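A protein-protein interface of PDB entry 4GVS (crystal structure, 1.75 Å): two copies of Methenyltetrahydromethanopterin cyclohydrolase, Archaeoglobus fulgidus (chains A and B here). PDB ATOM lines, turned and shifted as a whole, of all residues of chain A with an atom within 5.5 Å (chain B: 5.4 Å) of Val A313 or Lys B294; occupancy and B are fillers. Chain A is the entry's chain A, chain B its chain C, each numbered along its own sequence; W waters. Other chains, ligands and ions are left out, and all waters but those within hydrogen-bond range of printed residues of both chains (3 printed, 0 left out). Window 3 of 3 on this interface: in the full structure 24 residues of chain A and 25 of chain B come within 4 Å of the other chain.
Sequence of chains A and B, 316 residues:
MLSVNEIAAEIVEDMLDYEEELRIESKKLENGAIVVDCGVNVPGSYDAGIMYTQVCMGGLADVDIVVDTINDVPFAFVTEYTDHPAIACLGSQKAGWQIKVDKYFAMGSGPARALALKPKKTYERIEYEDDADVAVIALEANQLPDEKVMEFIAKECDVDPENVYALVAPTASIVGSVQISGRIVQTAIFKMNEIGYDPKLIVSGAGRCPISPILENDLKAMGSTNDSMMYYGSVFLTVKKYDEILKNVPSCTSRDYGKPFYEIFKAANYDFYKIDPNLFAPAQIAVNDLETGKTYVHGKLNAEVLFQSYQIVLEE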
ATOM      1  N   ILE A 214     -14.091 -20.700 -16.297  1.00  0.00           N
ATOM      2  CA  ILE A 214     -13.670 -19.998 -15.095  1.00  0.00           C
ATOM      3  C   ILE A 214     -13.548 -18.513 -15.431  1.00  0.00           C
ATOM      4  O   ILE A 214     -12.769 -18.118 -16.323  1.00  0.00           O
ATOM      5  CB  ILE A 214     -12.322 -20.520 -14.545  1.00  0.00           C
ATOM      6  CG1 ILE A 214     -12.420 -22.029 -14.179  1.00  0.00           C
ATOM      7  CG2 ILE A 214     -11.982 -19.728 -13.288  1.00  0.00           C
ATOM      8  CD1 ILE A 214     -11.104 -22.783 -14.212  1.00  0.00           C
ATOM      9  N   GLU A 216     -13.097 -14.326 -14.041  1.00  0.00           N
ATOM     10  CA  GLU A 216     -11.885 -13.683 -13.587  1.00  0.00           C
ATOM     11  C   GLU A 216     -11.880 -13.435 -12.079  1.00  0.00           C
ATOM     12  O   GLU A 216     -10.839 -13.108 -11.535  1.00  0.00           O
ATOM     13  CB  GLU A 216     -11.570 -12.433 -14.449  1.00  0.00           C
ATOM     14  CG  GLU A 216     -12.508 -11.254 -14.206  1.00  0.00           C
ATOM     15  CD  GLU A 216     -13.708 -11.197 -15.140  1.00  0.00           C
ATOM     16  OE1 GLU A 216     -14.226 -12.257 -15.597  1.00  0.00           O
ATOM     17  OE2 GLU A 216     -14.163 -10.064 -15.395  1.00  0.00           O
ATOM     18  N   TYR A 310     -21.344 -16.544 -19.741  1.00  0.00           N
ATOM     19  CA  TYR A 310     -20.054 -17.181 -19.960  1.00  0.00           C
ATOM     20  C   TYR A 310     -18.957 -16.297 -20.572  1.00  0.00           C
ATOM     21  O   TYR A 310     -17.810 -16.742 -20.703  1.00  0.00           O
ATOM     22  CB  TYR A 310     -20.256 -18.388 -20.874  1.00  0.00           C
ATOM     23  CG  TYR A 310     -20.778 -19.635 -20.170  1.00  0.00           C
ATOM     24  CD1 TYR A 310     -21.227 -19.635 -18.860  1.00  0.00           C
ATOM     25  CD2 TYR A 310     -20.785 -20.876 -20.876  1.00  0.00           C
ATOM     26  CE1 TYR A 310     -21.673 -20.811 -18.240  1.00  0.00           C
ATOM     27  CE2 TYR A 310     -21.245 -22.034 -20.292  1.00  0.00           C
ATOM     28  CZ  TYR A 310     -21.691 -22.014 -18.988  1.00  0.00           C
ATOM     29  OH  TYR A 310     -22.108 -23.186 -18.405  1.00  0.00           O
ATOM     30  N   GLN A 311     -19.308 -15.076 -21.006  1.00  0.00           N
ATOM     31  CA  GLN A 311     -18.337 -14.125 -21.590  1.00  0.00           C
ATOM     32  C   GLN A 311     -17.669 -14.726 -22.787  1.00  0.00           C
ATOM     33  O   GLN A 311     -16.434 -14.626 -22.997  1.00  0.00           O
ATOM     34  CB  GLN A 311     -17.318 -13.665 -20.544  1.00  0.00           C
ATOM     35  CG  GLN A 311     -18.003 -13.086 -19.301  1.00  0.00           C
ATOM     36  CD  GLN A 311     -17.084 -12.359 -18.342  1.00  0.00           C
ATOM     37  OE1 GLN A 311     -15.908 -12.688 -18.184  1.00  0.00           O
ATOM     38  NE2 GLN A 311     -17.631 -11.373 -17.668  1.00  0.00           N
ATOM     39  N   ILE A 312     -18.533 -15.358 -23.577  1.00  0.00           N
ATOM     40  CA  ILE A 312     -18.155 -15.888 -24.862  1.00  0.00           C
ATOM     41  C   ILE A 312     -17.830 -14.801 -25.871  1.00  0.00           C
ATOM     42  O   ILE A 312     -18.593 -13.832 -26.038  1.00  0.00           O
ATOM     43  CB  ILE A 312     -19.291 -16.768 -25.415  1.00  0.00           C
ATOM     44  CG1 ILE A 312     -19.463 -18.006 -24.513  1.00  0.00           C
ATOM     45  CG2 ILE A 312     -19.003 -17.216 -26.822  1.00  0.00           C
ATOM     46  CD1 ILE A 312     -18.270 -18.989 -24.605  1.00  0.00           C
ATOM     47  N   VAL A 313     -16.713 -14.991 -26.557  1.00  0.00           N
ATOM     48  CA  VAL A 313     -16.265 -14.111 -27.626  1.00  0.00           C
ATOM     49  C   VAL A 313     -16.203 -14.926 -28.883  1.00  0.00           C
ATOM     50  O   VAL A 313     -15.309 -15.745 -29.080  1.00  0.00           O
ATOM     51  CB  VAL A 313     -14.886 -13.446 -27.305  1.00  0.00           C
ATOM     52  CG1 VAL A 313     -14.417 -12.496 -28.415  1.00  0.00           C
ATOM     53  CG2 VAL A 313     -14.978 -12.715 -25.984  1.00  0.00           C
ATOM     54  N   LEU A 314     -17.177 -14.688 -29.750  1.00  0.00           N
ATOM     55  CA  LEU A 314     -17.197 -15.278 -31.058  1.00  0.00           C
ATOM     56  C   LEU A 314     -16.484 -14.407 -32.035  1.00  0.00           C
ATOM     57  O   LEU A 314     -16.233 -13.242 -31.765  1.00  0.00           O
ATOM     58  CB  LEU A 314     -18.650 -15.412 -31.557  1.00  0.00           C
ATOM     59  CG  LEU A 314     -19.648 -16.110 -30.635  1.00  0.00           C
ATOM     60  CD1 LEU A 314     -21.051 -15.896 -31.196  1.00  0.00           C
ATOM     61  CD2 LEU A 314     -19.282 -17.586 -30.590  1.00  0.00           C
ATOM     62  N   GLU A 315     -16.159 -14.975 -33.187  1.00  0.00           N
ATOM     63  CA  GLU A 315     -15.544 -14.199 -34.237  1.00  0.00           C
ATOM     64  C   GLU A 315     -16.657 -13.474 -34.987  1.00  0.00           C
ATOM     65  O   GLU A 315     -16.396 -12.452 -35.616  1.00  0.00           O
ATOM     66  CB  GLU A 315     -14.754 -15.084 -35.185  1.00  0.00           C
ATOM     67  CG  GLU A 315     -13.528 -15.722 -34.568  1.00  0.00           C
ATOM     68  CD  GLU A 315     -12.838 -16.661 -35.532  1.00  0.00           C
ATOM     69  OE1 GLU A 315     -13.301 -16.787 -36.695  1.00  0.00           O
ATOM     70  OE2 GLU A 315     -11.829 -17.283 -35.152  1.00  0.00           O
ATOM     71  N   VAL B 287     -11.632 -21.327 -26.025  1.00  0.00           N
ATOM     72  CA  VAL B 287     -10.433 -21.123 -25.134  1.00  0.00           C
ATOM     73  C   VAL B 287     -10.805 -20.186 -23.998  1.00  0.00           C
ATOM     74  O   VAL B 287     -10.976 -18.971 -24.210  1.00  0.00           O
ATOM     75  CB  VAL B 287      -9.186 -20.574 -25.915  1.00  0.00           C
ATOM     76  CG1 VAL B 287      -7.913 -20.571 -25.031  1.00  0.00           C
ATOM     77  CG2 VAL B 287      -8.947 -21.319 -27.222  1.00  0.00           C
ATOM     78  N   ASN B 288     -10.925 -20.778 -22.811  1.00  0.00           N
ATOM     79  CA  ASN B 288     -11.263 -20.067 -21.587  1.00  0.00           C
ATOM     80  C   ASN B 288      -9.947 -19.459 -21.128  1.00  0.00           C
ATOM     81  O   ASN B 288      -9.032 -20.173 -20.689  1.00  0.00           O
ATOM     82  CB  ASN B 288     -11.822 -21.045 -20.529  1.00  0.00           C
ATOM     83  CG  ASN B 288     -12.044 -20.402 -19.176  1.00  0.00           C
ATOM     84  OD1 ASN B 288     -12.196 -19.157 -19.060  1.00  0.00           O
ATOM     85  ND2 ASN B 288     -12.072 -21.218 -18.150  1.00  0.00           N
ATOM     86  N   ASP B 289      -9.884 -18.127 -21.217  1.00  0.00           N
ATOM     87  CA  ASP B 289      -8.756 -17.321 -20.702  1.00  0.00           C
ATOM     88  C   ASP B 289      -8.871 -17.001 -19.201  1.00  0.00           C
ATOM     89  O   ASP B 289      -9.775 -16.263 -18.760  1.00  0.00           O
ATOM     90  CB  ASP B 289      -8.734 -16.011 -21.514  1.00  0.00           C
ATOM     91  CG  ASP B 289      -7.539 -15.118 -21.182  1.00  0.00           C
ATOM     92  OD1 ASP B 289      -6.556 -15.642 -20.680  1.00  0.00           O
ATOM     93  OD2 ASP B 289      -7.635 -13.888 -21.414  1.00  0.00           O
ATOM     94  N   THR B 292      -8.487 -12.762 -18.532  1.00  0.00           N
ATOM     95  CA  THR B 292      -9.602 -11.863 -18.790  1.00  0.00           C
ATOM     96  C   THR B 292     -10.926 -12.477 -18.316  1.00  0.00           C
ATOM     97  O   THR B 292     -11.882 -11.739 -18.020  1.00  0.00           O
ATOM     98  CB  THR B 292      -9.697 -11.559 -20.280  1.00  0.00           C
ATOM     99  OG1 THR B 292      -9.944 -12.793 -20.985  1.00  0.00           O
ATOM    100  CG2 THR B 292      -8.339 -10.987 -20.780  1.00  0.00           C
ATOM    101  N   GLY B 293     -10.964 -13.807 -18.158  1.00  0.00           N
ATOM    102  CA  GLY B 293     -12.214 -14.486 -17.805  1.00  0.00           C
ATOM    103  C   GLY B 293     -13.163 -14.623 -18.991  1.00  0.00           C
ATOM    104  O   GLY B 293     -14.350 -14.995 -18.797  1.00  0.00           O
ATOM    105  N   LYS B 294     -12.669 -14.325 -20.196  1.00  0.00           N
ATOM    106  CA  LYS B 294     -13.422 -14.516 -21.429  1.00  0.00           C
ATOM    107  C   LYS B 294     -13.120 -15.877 -22.065  1.00  0.00           C
ATOM    108  O   LYS B 294     -12.103 -16.491 -21.784  1.00  0.00           O
ATOM    109  CB  LYS B 294     -13.102 -13.457 -22.485  1.00  0.00           C
ATOM    110  CG  LYS B 294     -13.374 -12.012 -22.083  1.00  0.00           C
ATOM    111  CD  LYS B 294     -13.173 -11.180 -23.335  1.00  0.00           C
ATOM    112  CE  LYS B 294     -12.707  -9.765 -23.055  1.00  0.00           C
ATOM    113  NZ  LYS B 294     -13.708  -9.176 -22.138  1.00  0.00           N
ATOM    114  N   THR B 295     -14.000 -16.319 -22.940  1.00  0.00           N
ATOM    115  CA  THR B 295     -13.775 -17.607 -23.611  1.00  0.00           C
ATOM    116  C   THR B 295     -13.929 -17.381 -25.085  1.00  0.00           C
ATOM    117  O   THR B 295     -15.010 -17.008 -25.574  1.00  0.00           O
ATOM    118  CB  THR B 295     -14.750 -18.740 -23.162  1.00  0.00           C
ATOM    119  OG1 THR B 295     -14.402 -19.141 -21.834  1.00  0.00           O
ATOM    120  CG2 THR B 295     -14.565 -19.983 -24.052  1.00  0.00           C
ATOM    121  N   TYR B 296     -12.851 -17.625 -25.791  1.00  0.00           N
ATOM    122  CA  TYR B 296     -12.722 -17.289 -27.224  1.00  0.00           C
ATOM    123  C   TYR B 296     -12.980 -18.478 -28.123  1.00  0.00           C
ATOM    124  O   TYR B 296     -12.292 -19.491 -28.006  1.00  0.00           O
ATOM    125  CB  TYR B 296     -11.300 -16.805 -27.523  1.00  0.00           C
ATOM    126  CG  TYR B 296     -10.989 -15.502 -26.892  1.00  0.00           C
ATOM    127  CD1 TYR B 296     -10.525 -15.441 -25.575  1.00  0.00           C
ATOM    128  CD2 TYR B 296     -11.171 -14.286 -27.622  1.00  0.00           C
ATOM    129  CE1 TYR B 296     -10.225 -14.207 -24.986  1.00  0.00           C
ATOM    130  CE2 TYR B 296     -10.872 -13.064 -27.030  1.00  0.00           C
ATOM    131  CZ  TYR B 296     -10.410 -13.038 -25.727  1.00  0.00           C
ATOM    132  OH  TYR B 296     -10.110 -11.839 -25.125  1.00  0.00           O
ATOM    133  N   VAL B 297     -13.912 -18.350 -29.066  1.00  0.00           N
ATOM    134  CA  VAL B 297     -14.299 -19.492 -29.908  1.00  0.00           C
ATOM    135  C   VAL B 297     -13.744 -19.273 -31.344  1.00  0.00           C
ATOM    136  O   VAL B 297     -13.867 -18.186 -31.904  1.00  0.00           O
ATOM    137  CB  VAL B 297     -15.850 -19.653 -30.024  1.00  0.00           C
ATOM    138  CG1 VAL B 297     -16.190 -20.889 -30.864  1.00  0.00           C
ATOM    139  CG2 VAL B 297     -16.475 -19.760 -28.620  1.00  0.00           C
HETATM  140  O   HOH W   1     -16.446 -17.805 -33.654  1.00  0.00           O
HETATM  141  O   HOH W   2     -15.311 -17.239 -20.006  1.00  0.00           O
HETATM  142  O   HOH W   3     -13.145 -15.670 -30.815  1.00  0.00           O
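The backbone NH of Val B297 lies within hydrogen-bond range of the backbone carbonyl oxygen of Val A313. The backbone carbonyl oxygen (O) of Gln A311 sits at hydrogen-bond distance from the backbone NH (N) of Thr B295, 3.0 Å away. N of Val A313 is in hydrogen-bond range of O of Thr B295. OE1 of Gln A311 sits close to O of Gly B293. OE1 of Glu A216 sits close to O of Thr B292 (3.4 Å). The backbone NH (N) of Ile A214 sits close to the side-chain amide nitrogen (ND2) of Asn B288 (2.8 Å).
N of Lys B294 sits close to OG1 of Thr B292, at 3.2 Å. The side-chain hydroxyl (OG1) of Thr B292 sits at hydrogen-bond distance from the side-chain carboxylate (OD2) of Asp B289 (2.6 Å). The backbone NH of Val B287 is in hydrogen-bond range of the backbone carbonyl oxygen of Tyr B296. N of Asp B289 is in hydrogen-bond range of O of Lys B294. The side-chain carboxylate (OE1) of Glu A216 lies close to the side-chain amide oxygen (OE1) of Gln A311, at 3.1 Å.
O of Ile A214 touches CA of Gly B293, at 3.96 Å. Glu A216 touches Gly B293. O of Gln A311 touches CA of Lys B294 (3.4 Å). Ile A312 touches Thr B295. Val A313 touches Lys B294. Tyr B296 touches Val A313 (CA to O, 3.5 Å). Val B297 touches Glu A315.
Val A313 touches four residues of chain B. Of the printed residues of chain B, Glu A315 touches Val B297 (3.6 Å). Printed residues of chain A within 4 Å of Thr B292: Glu A216 (3.4 Å). Of the printed residues of chain A, Lys B294 touches Gln A311 (3.4 Å) and Val A313 (3.6 Å). Printed residues of chain A within 4 Å of Thr B295: Gln A311 (3.0 Å), Ile A312 (3.4 Å) and Val A313 (2.8 Å). The nearest printed residue of chain B that does not touch Val A313 is Thr B292 (7.1 Å). The nearest printed residue of chain B that does not touch Ile A214 is Asp B289 (4.3 Å).
Of the 9 printed residues of chain B, 7 touch a printed residue of chain A. Hydrophobic or aromatic side chains of chain B within 4 Å of the printed part of chain A: Tyr B296. Printed residues of chain A that touch a printed residue of chain B: Ile A214, Glu A216, Gln A311, Ile A312, Val A313 and Glu A315.
No position is printed for both chains.
Water W2 lies within hydrogen-bond range of O of Tyr A310, O of Gly B293 and OG1 of Thr B295. Water W3 lies within hydrogen-bond range of the backbone carbonyl oxygen of Val A313 (2.8 Å) and the backbone carbonyl oxygen of Val B297 (2.8 Å). Water W1 bridges N of Glu A315 (2.9 Å) and O of Val B297 (3.1 Å).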
